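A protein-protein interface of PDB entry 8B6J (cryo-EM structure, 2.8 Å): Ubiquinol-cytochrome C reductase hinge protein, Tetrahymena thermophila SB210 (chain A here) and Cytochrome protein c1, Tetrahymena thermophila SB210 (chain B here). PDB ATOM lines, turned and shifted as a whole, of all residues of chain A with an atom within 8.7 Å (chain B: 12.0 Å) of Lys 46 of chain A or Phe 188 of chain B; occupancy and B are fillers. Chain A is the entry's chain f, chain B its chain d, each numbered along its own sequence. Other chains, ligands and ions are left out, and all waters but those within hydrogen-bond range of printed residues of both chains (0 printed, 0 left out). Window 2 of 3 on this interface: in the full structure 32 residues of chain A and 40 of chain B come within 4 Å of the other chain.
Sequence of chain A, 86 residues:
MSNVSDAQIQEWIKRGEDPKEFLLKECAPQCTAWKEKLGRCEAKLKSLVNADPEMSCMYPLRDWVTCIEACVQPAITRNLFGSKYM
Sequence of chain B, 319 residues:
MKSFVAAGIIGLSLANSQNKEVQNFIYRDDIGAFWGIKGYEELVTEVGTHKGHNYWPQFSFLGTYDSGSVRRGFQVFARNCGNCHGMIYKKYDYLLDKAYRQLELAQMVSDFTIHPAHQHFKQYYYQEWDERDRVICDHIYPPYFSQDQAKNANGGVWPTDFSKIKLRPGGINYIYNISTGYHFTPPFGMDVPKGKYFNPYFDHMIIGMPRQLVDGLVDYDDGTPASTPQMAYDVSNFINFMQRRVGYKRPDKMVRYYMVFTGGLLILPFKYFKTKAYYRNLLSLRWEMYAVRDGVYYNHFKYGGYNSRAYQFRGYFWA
Pro 187 of chain B touches Glu 42 of chain A.
Leu 45 of chain A touches Phe 188 of chain B (CD2 to CE2, 3.4 Å).
Lys 46 of chain A touches Phe 188 of chain B.
O of Cys 57 of chain A touches CG of Pro 187 of chain B, at 3.0 Å.
CG of Met 58 of chain A touches SD of Met 190 of chain B (3.98 Å).
Met 58 of chain A touches His 204 of chain B.
Met 58 of chain A touches Met 205 of chain B (CE to CG, 3.6 Å).
Pro 187 of chain B touches Leu 61 of chain A (CD to CD1, 3.6 Å).
Leu 61 of chain A touches Phe 198 of chain B.
Met 205 of chain B touches Leu 61 of chain A.
The side-chain sulfur (SG) of Cys 57 of chain A sits at hydrogen-bond distance from the backbone carbonyl oxygen (O) of Phe 188 of chain B (3.4 Å).
No residue of chain B comes within 4 Å of Ala 43 of chain A.
Of chain B, only Phe 188 (3.4 Å) comes within 4 Å of Leu 45 of chain A.
Printed residues of chain B within 4 Å of Lys 46 of chain A: Phe 188 (3.4 Å).
No residue of chain B comes within 4 Å of Ser 47 of chain A.
No residue of chain B comes within 4 Å of Leu 48 of chain A.
No residue of chain B comes within 4 Å of Val 49 of chain A.
Of chain B, only Pro 187 and Phe 188 come within 4 Å of Cys 57 of chain A.
Printed residues of chain B within 4 Å of Met 58 of chain A: Met 190, His 204 and Met 205.
Of the printed residues of chain B, Leu 61 of chain A touches Thr 185 (3.8 Å), Pro 187 (3.6 Å), Phe 198 (3.8 Å) and Met 205 (3.7 Å).
Of chain A, only Glu 42, Cys 57 and Leu 61 come within 4 Å of Pro 187 of chain B.
Phe 188 of chain B touches four residues of chain A.
Asp 191 of chain B touches none of the printed residues of chain A.
Of the printed residues of chain A, Phe 198 of chain B touches Leu 61 (3.8 Å).
Of the printed residues of chain A, Met 205 of chain B touches Met 58 and Leu 61.
The nearest printed residue of chain A that does not touch Phe 198 of chain B is Met 58 of chain A (6.2 Å).
Hydrophobic or aromatic side chains of chain A within 4 Å of the printed part of chain B: Leu 45, Met 58 and Leu 61.
Along chain A the printed residues that touch a printed residue of chain B span positions 42 to 61.
Of the 13 printed residues of chain B, 7 touch a printed residue of chain A.
Hydrophobic or aromatic side chains of chain B that line the printed part of chain A: Pro 187, Phe 188, Met 190, Phe 198 and Met 205.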
ATOM      1  N   LEU A  38      -1.145  -0.518 -17.473  1.00  0.00           N
ATOM      2  CA  LEU A  38       0.006  -0.686 -16.592  1.00  0.00           C
ATOM      3  C   LEU A  38      -0.226  -1.814 -15.595  1.00  0.00           C
ATOM      4  O   LEU A  38       0.680  -2.612 -15.324  1.00  0.00           O
ATOM      5  CB  LEU A  38       0.299   0.624 -15.862  1.00  0.00           C
ATOM      6  CG  LEU A  38       1.428   0.589 -14.830  1.00  0.00           C
ATOM      7  CD1 LEU A  38       2.739   0.167 -15.470  1.00  0.00           C
ATOM      8  CD2 LEU A  38       1.569   1.943 -14.160  1.00  0.00           C
ATOM      9  N   GLY A  39      -1.431  -1.889 -15.028  1.00  0.00           N
ATOM     10  CA  GLY A  39      -1.732  -2.975 -14.109  1.00  0.00           C
ATOM     11  C   GLY A  39      -1.617  -4.338 -14.766  1.00  0.00           C
ATOM     12  O   GLY A  39      -1.049  -5.271 -14.191  1.00  0.00           O
ATOM     13  N   ARG A  40      -2.150  -4.471 -15.981  1.00  0.00           N
ATOM     14  CA  ARG A  40      -2.054  -5.740 -16.694  1.00  0.00           C
ATOM     15  C   ARG A  40      -0.606  -6.078 -17.025  1.00  0.00           C
ATOM     16  O   ARG A  40      -0.196  -7.242 -16.942  1.00  0.00           O
ATOM     17  CB  ARG A  40      -2.904  -5.696 -17.964  1.00  0.00           C
ATOM     18  CG  ARG A  40      -4.397  -5.781 -17.695  1.00  0.00           C
ATOM     19  CD  ARG A  40      -5.208  -5.903 -18.976  1.00  0.00           C
ATOM     20  NE  ARG A  40      -5.299  -4.640 -19.700  1.00  0.00           N
ATOM     21  CZ  ARG A  40      -4.492  -4.272 -20.687  1.00  0.00           C
ATOM     22  NH1 ARG A  40      -3.503  -5.048 -21.103  1.00  0.00           N
ATOM     23  NH2 ARG A  40      -4.686  -3.096 -21.276  1.00  0.00           N
ATOM     24  N   CYS A  41       0.183  -5.072 -17.411  1.00  0.00           N
ATOM     25  CA  CYS A  41       1.593  -5.316 -17.694  1.00  0.00           C
ATOM     26  C   CYS A  41       2.321  -5.808 -16.451  1.00  0.00           C
ATOM     27  O   CYS A  41       3.119  -6.752 -16.521  1.00  0.00           O
ATOM     28  CB  CYS A  41       2.244  -4.042 -18.230  1.00  0.00           C
ATOM     29  SG  CYS A  41       3.988  -4.222 -18.664  1.00  0.00           S
ATOM     30  N   GLU A  42       2.057  -5.184 -15.301  1.00  0.00           N
ATOM     31  CA  GLU A  42       2.682  -5.633 -14.062  1.00  0.00           C
ATOM     32  C   GLU A  42       2.254  -7.052 -13.715  1.00  0.00           C
ATOM     33  O   GLU A  42       3.078  -7.873 -13.295  1.00  0.00           O
ATOM     34  CB  GLU A  42       2.343  -4.678 -12.919  1.00  0.00           C
ATOM     35  CG  GLU A  42       3.014  -3.321 -13.029  1.00  0.00           C
ATOM     36  CD  GLU A  42       2.854  -2.489 -11.773  1.00  0.00           C
ATOM     37  OE1 GLU A  42       2.480  -3.056 -10.725  1.00  0.00           O
ATOM     38  OE2 GLU A  42       3.100  -1.266 -11.832  1.00  0.00           O
ATOM     39  N   ALA A  43       0.968  -7.361 -13.883  1.00  0.00           N
ATOM     40  CA  ALA A  43       0.495  -8.712 -13.604  1.00  0.00           C
ATOM     41  C   ALA A  43       1.223  -9.730 -14.473  1.00  0.00           C
ATOM     42  O   ALA A  43       1.719 -10.749 -13.976  1.00  0.00           O
ATOM     43  CB  ALA A  43      -1.015  -8.794 -13.825  1.00  0.00           C
ATOM     44  N   LYS A  44       1.309  -9.465 -15.779  1.00  0.00           N
ATOM     45  CA  LYS A  44       1.980 -10.412 -16.663  1.00  0.00           C
ATOM     46  C   LYS A  44       3.450 -10.557 -16.298  1.00  0.00           C
ATOM     47  O   LYS A  44       3.980 -11.674 -16.268  1.00  0.00           O
ATOM     48  CB  LYS A  44       1.841  -9.986 -18.124  1.00  0.00           C
ATOM     49  CG  LYS A  44       2.622 -10.895 -19.066  1.00  0.00           C
ATOM     50  CD  LYS A  44       2.276 -10.678 -20.524  1.00  0.00           C
ATOM     51  CE  LYS A  44       3.063 -11.639 -21.407  1.00  0.00           C
ATOM     52  NZ  LYS A  44       2.740 -11.505 -22.854  1.00  0.00           N
ATOM     53  N   LEU A  45       4.131  -9.444 -16.016  1.00  0.00           N
ATOM     54  CA  LEU A  45       5.546  -9.532 -15.677  1.00  0.00           C
ATOM     55  C   LEU A  45       5.749 -10.326 -14.393  1.00  0.00           C
ATOM     56  O   LEU A  45       6.739 -11.053 -14.254  1.00  0.00           O
ATOM     57  CB  LEU A  45       6.150  -8.135 -15.551  1.00  0.00           C
ATOM     58  CG  LEU A  45       7.672  -8.129 -15.393  1.00  0.00           C
ATOM     59  CD1 LEU A  45       8.308  -7.081 -16.290  1.00  0.00           C
ATOM     60  CD2 LEU A  45       8.058  -7.897 -13.946  1.00  0.00           C
ATOM     61  N   LYS A  46       4.821 -10.199 -13.441  1.00  0.00           N
ATOM     62  CA  LYS A  46       4.872 -11.044 -12.253  1.00  0.00           C
ATOM     63  C   LYS A  46       4.691 -12.513 -12.617  1.00  0.00           C
ATOM     64  O   LYS A  46       5.375 -13.385 -12.070  1.00  0.00           O
ATOM     65  CB  LYS A  46       3.804 -10.612 -11.250  1.00  0.00           C
ATOM     66  CG  LYS A  46       4.104  -9.306 -10.541  1.00  0.00           C
ATOM     67  CD  LYS A  46       2.974  -8.918  -9.598  1.00  0.00           C
ATOM     68  CE  LYS A  46       3.275  -7.614  -8.878  1.00  0.00           C
ATOM     69  NZ  LYS A  46       2.145  -7.178  -8.014  1.00  0.00           N
ATOM     70  N   SER A  47       3.770 -12.805 -13.538  1.00  0.00           N
ATOM     71  CA  SER A  47       3.481 -14.196 -13.876  1.00  0.00           C
ATOM     72  C   SER A  47       4.695 -14.886 -14.485  1.00  0.00           C
ATOM     73  O   SER A  47       4.971 -16.053 -14.183  1.00  0.00           O
ATOM     74  CB  SER A  47       2.292 -14.268 -14.835  1.00  0.00           C
ATOM     75  OG  SER A  47       2.648 -13.814 -16.128  1.00  0.00           O
ATOM     76  N   LEU A  48       5.427 -14.189 -15.351  1.00  0.00           N
ATOM     77  CA  LEU A  48       6.559 -14.798 -16.036  1.00  0.00           C
ATOM     78  C   LEU A  48       7.604 -15.282 -15.038  1.00  0.00           C
ATOM     79  O   LEU A  48       7.867 -14.633 -14.022  1.00  0.00           O
ATOM     80  CB  LEU A  48       7.193 -13.799 -17.004  1.00  0.00           C
ATOM     81  CG  LEU A  48       6.319 -13.326 -18.165  1.00  0.00           C
ATOM     82  CD1 LEU A  48       7.065 -12.301 -19.001  1.00  0.00           C
ATOM     83  CD2 LEU A  48       5.878 -14.498 -19.026  1.00  0.00           C
ATOM     84  N   VAL A  49       8.198 -16.434 -15.335  1.00  0.00           N
ATOM     85  CA  VAL A  49       9.262 -16.999 -14.516  1.00  0.00           C
ATOM     86  C   VAL A  49      10.637 -16.714 -15.108  1.00  0.00           C
ATOM     87  O   VAL A  49      11.567 -16.364 -14.380  1.00  0.00           O
ATOM     88  CB  VAL A  49       9.039 -18.516 -14.326  1.00  0.00           C
ATOM     89  CG1 VAL A  49       9.198 -19.264 -15.645  1.00  0.00           C
ATOM     90  CG2 VAL A  49       9.991 -19.064 -13.274  1.00  0.00           C
ATOM     91  N   ASN A  50      10.786 -16.859 -16.426  1.00  0.00           N
ATOM     92  CA  ASN A  50      12.027 -16.518 -17.119  1.00  0.00           C
ATOM     93  C   ASN A  50      11.843 -15.138 -17.744  1.00  0.00           C
ATOM     94  O   ASN A  50      11.543 -14.990 -18.929  1.00  0.00           O
ATOM     95  CB  ASN A  50      12.375 -17.573 -18.165  1.00  0.00           C
ATOM     96  CG  ASN A  50      12.682 -18.926 -17.552  1.00  0.00           C
ATOM     97  OD1 ASN A  50      11.996 -19.911 -17.823  1.00  0.00           O
ATOM     98  ND2 ASN A  50      13.719 -18.979 -16.725  1.00  0.00           N
ATOM     99  N   ALA A  51      12.029 -14.112 -16.920  1.00  0.00           N
ATOM    100  CA  ALA A  51      11.811 -12.733 -17.337  1.00  0.00           C
ATOM    101  C   ALA A  51      13.085 -12.188 -17.969  1.00  0.00           C
ATOM    102  O   ALA A  51      14.129 -12.112 -17.312  1.00  0.00           O
ATOM    103  CB  ALA A  51      11.389 -11.871 -16.148  1.00  0.00           C
ATOM    104  N   MET A  55      12.591  -6.739 -20.363  1.00  0.00           N
ATOM    105  CA  MET A  55      11.189  -6.547 -20.014  1.00  0.00           C
ATOM    106  C   MET A  55      11.063  -5.739 -18.730  1.00  0.00           C
ATOM    107  O   MET A  55      11.746  -6.009 -17.739  1.00  0.00           O
ATOM    108  CB  MET A  55      10.499  -7.901 -19.855  1.00  0.00           C
ATOM    109  CG  MET A  55      10.371  -8.686 -21.149  1.00  0.00           C
ATOM    110  SD  MET A  55       9.472 -10.232 -20.930  1.00  0.00           S
ATOM    111  CE  MET A  55       9.431 -10.841 -22.612  1.00  0.00           C
ATOM    112  N   SER A  56      10.181  -4.742 -18.754  1.00  0.00           N
ATOM    113  CA  SER A  56       9.970  -3.884 -17.598  1.00  0.00           C
ATOM    114  C   SER A  56       8.628  -3.185 -17.742  1.00  0.00           C
ATOM    115  O   SER A  56       8.239  -2.800 -18.847  1.00  0.00           O
ATOM    116  CB  SER A  56      11.091  -2.848 -17.463  1.00  0.00           C
ATOM    117  OG  SER A  56      11.113  -1.978 -18.580  1.00  0.00           O
ATOM    118  N   CYS A  57       7.930  -3.021 -16.618  1.00  0.00           N
ATOM    119  CA  CYS A  57       6.676  -2.280 -16.603  1.00  0.00           C
ATOM    120  C   CYS A  57       6.970  -0.792 -16.497  1.00  0.00           C
ATOM    121  O   CYS A  57       6.438  -0.103 -15.620  1.00  0.00           O
ATOM    122  CB  CYS A  57       5.795  -2.736 -15.441  1.00  0.00           C
ATOM    123  SG  CYS A  57       5.897  -4.500 -15.100  1.00  0.00           S
ATOM    124  N   MET A  58       7.814  -0.289 -17.393  1.00  0.00           N
ATOM    125  CA  MET A  58       8.305   1.080 -17.352  1.00  0.00           C
ATOM    126  C   MET A  58       7.673   1.952 -18.423  1.00  0.00           C
ATOM    127  O   MET A  58       7.234   3.070 -18.140  1.00  0.00           O
ATOM    128  CB  MET A  58       9.830   1.075 -17.517  1.00  0.00           C
ATOM    129  CG  MET A  58      10.500   2.411 -17.284  1.00  0.00           C
ATOM    130  SD  MET A  58      12.278   2.305 -17.550  1.00  0.00           S
ATOM    131  CE  MET A  58      12.832   3.771 -16.693  1.00  0.00           C
ATOM    132  N   LEU A  61       4.033   2.690 -17.655  1.00  0.00           N
ATOM    133  CA  LEU A  61       3.994   3.688 -16.593  1.00  0.00           C
ATOM    134  C   LEU A  61       4.416   5.051 -17.119  1.00  0.00           C
ATOM    135  O   LEU A  61       3.884   6.079 -16.689  1.00  0.00           O
ATOM    136  CB  LEU A  61       4.886   3.266 -15.429  1.00  0.00           C
ATOM    137  CG  LEU A  61       5.011   4.318 -14.323  1.00  0.00           C
ATOM    138  CD1 LEU A  61       4.904   3.676 -12.955  1.00  0.00           C
ATOM    139  CD2 LEU A  61       6.316   5.082 -14.449  1.00  0.00           C
ATOM    140  N   PHE B 184       4.989  10.235  -7.801  1.00  0.00           N
ATOM    141  CA  PHE B 184       4.673   8.920  -8.335  1.00  0.00           C
ATOM    142  C   PHE B 184       5.556   7.848  -7.702  1.00  0.00           C
ATOM    143  O   PHE B 184       6.663   8.114  -7.225  1.00  0.00           O
ATOM    144  CB  PHE B 184       4.839   8.912  -9.853  1.00  0.00           C
ATOM    145  CG  PHE B 184       3.976   9.916 -10.557  1.00  0.00           C
ATOM    146  CD1 PHE B 184       2.690   9.590 -10.943  1.00  0.00           C
ATOM    147  CD2 PHE B 184       4.447  11.189 -10.828  1.00  0.00           C
ATOM    148  CE1 PHE B 184       1.892  10.511 -11.588  1.00  0.00           C
ATOM    149  CE2 PHE B 184       3.653  12.111 -11.472  1.00  0.00           C
ATOM    150  CZ  PHE B 184       2.374  11.771 -11.852  1.00  0.00           C
ATOM    151  N   THR B 185       5.046   6.609  -7.705  1.00  0.00           N
ATOM    152  CA  THR B 185       5.743   5.465  -7.137  1.00  0.00           C
ATOM    153  C   THR B 185       6.222   4.524  -8.241  1.00  0.00           C
ATOM    154  O   THR B 185       5.607   4.444  -9.307  1.00  0.00           O
ATOM    155  CB  THR B 185       4.842   4.682  -6.175  1.00  0.00           C
ATOM    156  OG1 THR B 185       3.669   4.237  -6.866  1.00  0.00           O
ATOM    157  CG2 THR B 185       4.436   5.552  -4.995  1.00  0.00           C
ATOM    158  N   PRO B 186       7.316   3.793  -8.014  1.00  0.00           N
ATOM    159  CA  PRO B 186       7.849   2.940  -9.072  1.00  0.00           C
ATOM    160  C   PRO B 186       6.924   1.770  -9.350  1.00  0.00           C
ATOM    161  O   PRO B 186       6.170   1.332  -8.464  1.00  0.00           O
ATOM    162  CB  PRO B 186       9.197   2.467  -8.499  1.00  0.00           C
ATOM    163  CG  PRO B 186       9.014   2.525  -7.033  1.00  0.00           C
ATOM    164  CD  PRO B 186       8.108   3.693  -6.775  1.00  0.00           C
ATOM    165  N   PRO B 187       6.943   1.232 -10.565  1.00  0.00           N
ATOM    166  CA  PRO B 187       6.159   0.033 -10.864  1.00  0.00           C
ATOM    167  C   PRO B 187       6.907  -1.226 -10.449  1.00  0.00           C
ATOM    168  O   PRO B 187       8.079  -1.195 -10.074  1.00  0.00           O
ATOM    169  CB  PRO B 187       5.992   0.103 -12.382  1.00  0.00           C
ATOM    170  CG  PRO B 187       7.252   0.753 -12.844  1.00  0.00           C
ATOM    171  CD  PRO B 187       7.685   1.703 -11.748  1.00  0.00           C
ATOM    172  N   PHE B 188       6.204  -2.352 -10.527  1.00  0.00           N
ATOM    173  CA  PHE B 188       6.839  -3.627 -10.230  1.00  0.00           C
ATOM    174  C   PHE B 188       7.933  -3.913 -11.250  1.00  0.00           C
ATOM    175  O   PHE B 188       7.811  -3.576 -12.431  1.00  0.00           O
ATOM    176  CB  PHE B 188       5.809  -4.756 -10.230  1.00  0.00           C
ATOM    177  CG  PHE B 188       6.396  -6.102  -9.919  1.00  0.00           C
ATOM    178  CD1 PHE B 188       6.587  -6.502  -8.609  1.00  0.00           C
ATOM    179  CD2 PHE B 188       6.768  -6.964 -10.936  1.00  0.00           C
ATOM    180  CE1 PHE B 188       7.130  -7.737  -8.319  1.00  0.00           C
ATOM    181  CE2 PHE B 188       7.313  -8.199 -10.651  1.00  0.00           C
ATOM    182  CZ  PHE B 188       7.495  -8.586  -9.343  1.00  0.00           C
ATOM    183  N   GLY B 189       9.011  -4.539 -10.786  1.00  0.00           N
ATOM    184  CA  GLY B 189      10.158  -4.822 -11.613  1.00  0.00           C
ATOM    185  C   GLY B 189      11.244  -3.768 -11.566  1.00  0.00           C
ATOM    186  O   GLY B 189      12.373  -4.043 -11.988  1.00  0.00           O
ATOM    187  N   MET B 190      10.939  -2.576 -11.063  1.00  0.00           N
ATOM    188  CA  MET B 190      11.924  -1.519 -10.887  1.00  0.00           C
ATOM    189  C   MET B 190      12.307  -1.433  -9.418  1.00  0.00           C
ATOM    190  O   MET B 190      11.439  -1.280  -8.552  1.00  0.00           O
ATOM    191  CB  MET B 190      11.380  -0.172 -11.364  1.00  0.00           C
ATOM    192  CG  MET B 190      11.332  -0.017 -12.875  1.00  0.00           C
ATOM    193  SD  MET B 190      10.792   1.624 -13.395  1.00  0.00           S
ATOM    194  CE  MET B 190      12.050   2.659 -12.651  1.00  0.00           C
ATOM    195  N   ASP B 191      13.602  -1.531  -9.143  1.00  0.00           N
ATOM    196  CA  ASP B 191      14.135  -1.443  -7.790  1.00  0.00           C
ATOM    197  C   ASP B 191      14.885  -0.129  -7.637  1.00  0.00           C
ATOM    198  O   ASP B 191      15.738   0.204  -8.466  1.00  0.00           O
ATOM    199  CB  ASP B 191      15.059  -2.623  -7.487  1.00  0.00           C
ATOM    200  CG  ASP B 191      16.151  -2.790  -8.525  1.00  0.00           C
ATOM    201  OD1 ASP B 191      16.057  -2.149  -9.592  1.00  0.00           O
ATOM    202  OD2 ASP B 191      17.102  -3.559  -8.273  1.00  0.00           O
ATOM    203  N   VAL B 192      14.566   0.612  -6.580  1.00  0.00           N
ATOM    204  CA  VAL B 192      15.207   1.890  -6.288  1.00  0.00           C
ATOM    205  C   VAL B 192      16.278   1.636  -5.228  1.00  0.00           C
ATOM    206  O   VAL B 192      15.929   1.349  -4.072  1.00  0.00           O
ATOM    207  CB  VAL B 192      14.188   2.932  -5.811  1.00  0.00           C
ATOM    208  CG1 VAL B 192      14.882   4.237  -5.460  1.00  0.00           C
ATOM    209  CG2 VAL B 192      13.127   3.158  -6.875  1.00  0.00           C
ATOM    210  N   PHE B 198      12.766   7.807  -7.019  1.00  0.00           N
ATOM    211  CA  PHE B 198      12.026   7.578  -8.252  1.00  0.00           C
ATOM    212  C   PHE B 198      11.457   8.898  -8.758  1.00  0.00           C
ATOM    213  O   PHE B 198      10.623   9.518  -8.090  1.00  0.00           O
ATOM    214  CB  PHE B 198      10.909   6.562  -8.023  1.00  0.00           C
ATOM    215  CG  PHE B 198      10.105   6.261  -9.251  1.00  0.00           C
ATOM    216  CD1 PHE B 198      10.634   5.488 -10.269  1.00  0.00           C
ATOM    217  CD2 PHE B 198       8.816   6.744  -9.386  1.00  0.00           C
ATOM    218  CE1 PHE B 198       9.895   5.208 -11.398  1.00  0.00           C
ATOM    219  CE2 PHE B 198       8.074   6.466 -10.513  1.00  0.00           C
ATOM    220  CZ  PHE B 198       8.615   5.698 -11.520  1.00  0.00           C
ATOM    221  N   HIS B 204      15.968   6.966 -17.069  1.00  0.00           N
ATOM    222  CA  HIS B 204      15.657   5.690 -16.434  1.00  0.00           C
ATOM    223  C   HIS B 204      14.840   5.855 -15.161  1.00  0.00           C
ATOM    224  O   HIS B 204      14.647   4.879 -14.427  1.00  0.00           O
ATOM    225  CB  HIS B 204      16.926   4.887 -16.132  1.00  0.00           C
ATOM    226  CG  HIS B 204      17.732   4.564 -17.350  1.00  0.00           C
ATOM    227  ND1 HIS B 204      17.472   3.470 -18.145  1.00  0.00           N
ATOM    228  CD2 HIS B 204      18.785   5.198 -17.916  1.00  0.00           C
ATOM    229  CE1 HIS B 204      18.333   3.441 -19.146  1.00  0.00           C
ATOM    230  NE2 HIS B 204      19.140   4.478 -19.031  1.00  0.00           N
ATOM    231  N   MET B 205      14.357   7.062 -14.877  1.00  0.00           N
ATOM    232  CA  MET B 205      13.414   7.324 -13.794  1.00  0.00           C
ATOM    233  C   MET B 205      14.002   7.052 -12.415  1.00  0.00           C
ATOM    234  O   MET B 205      13.258   6.822 -11.458  1.00  0.00           O
ATOM    235  CB  MET B 205      12.131   6.508 -13.978  1.00  0.00           C
ATOM    236  CG  MET B 205      11.441   6.738 -15.307  1.00  0.00           C
ATOM    237  SD  MET B 205       9.836   5.929 -15.387  1.00  0.00           S
ATOM    238  CE  MET B 205       9.247   6.511 -16.970  1.00  0.00           C
ATOM    239  N   ILE B 206      15.325   7.074 -12.281  1.00  0.00           N
ATOM    240  CA  ILE B 206      15.989   6.925 -10.989  1.00  0.00           C
ATOM    241  C   ILE B 206      16.991   8.062 -10.854  1.00  0.00           C
ATOM    242  O   ILE B 206      17.918   8.174 -11.664  1.00  0.00           O
ATOM    243  CB  ILE B 206      16.684   5.561 -10.847  1.00  0.00           C
ATOM    244  CG1 ILE B 206      15.672   4.432 -11.049  1.00  0.00           C
ATOM    245  CG2 ILE B 206      17.335   5.437  -9.478  1.00  0.00           C
ATOM    246  CD1 ILE B 206      16.275   3.046 -11.004  1.00  0.00           C
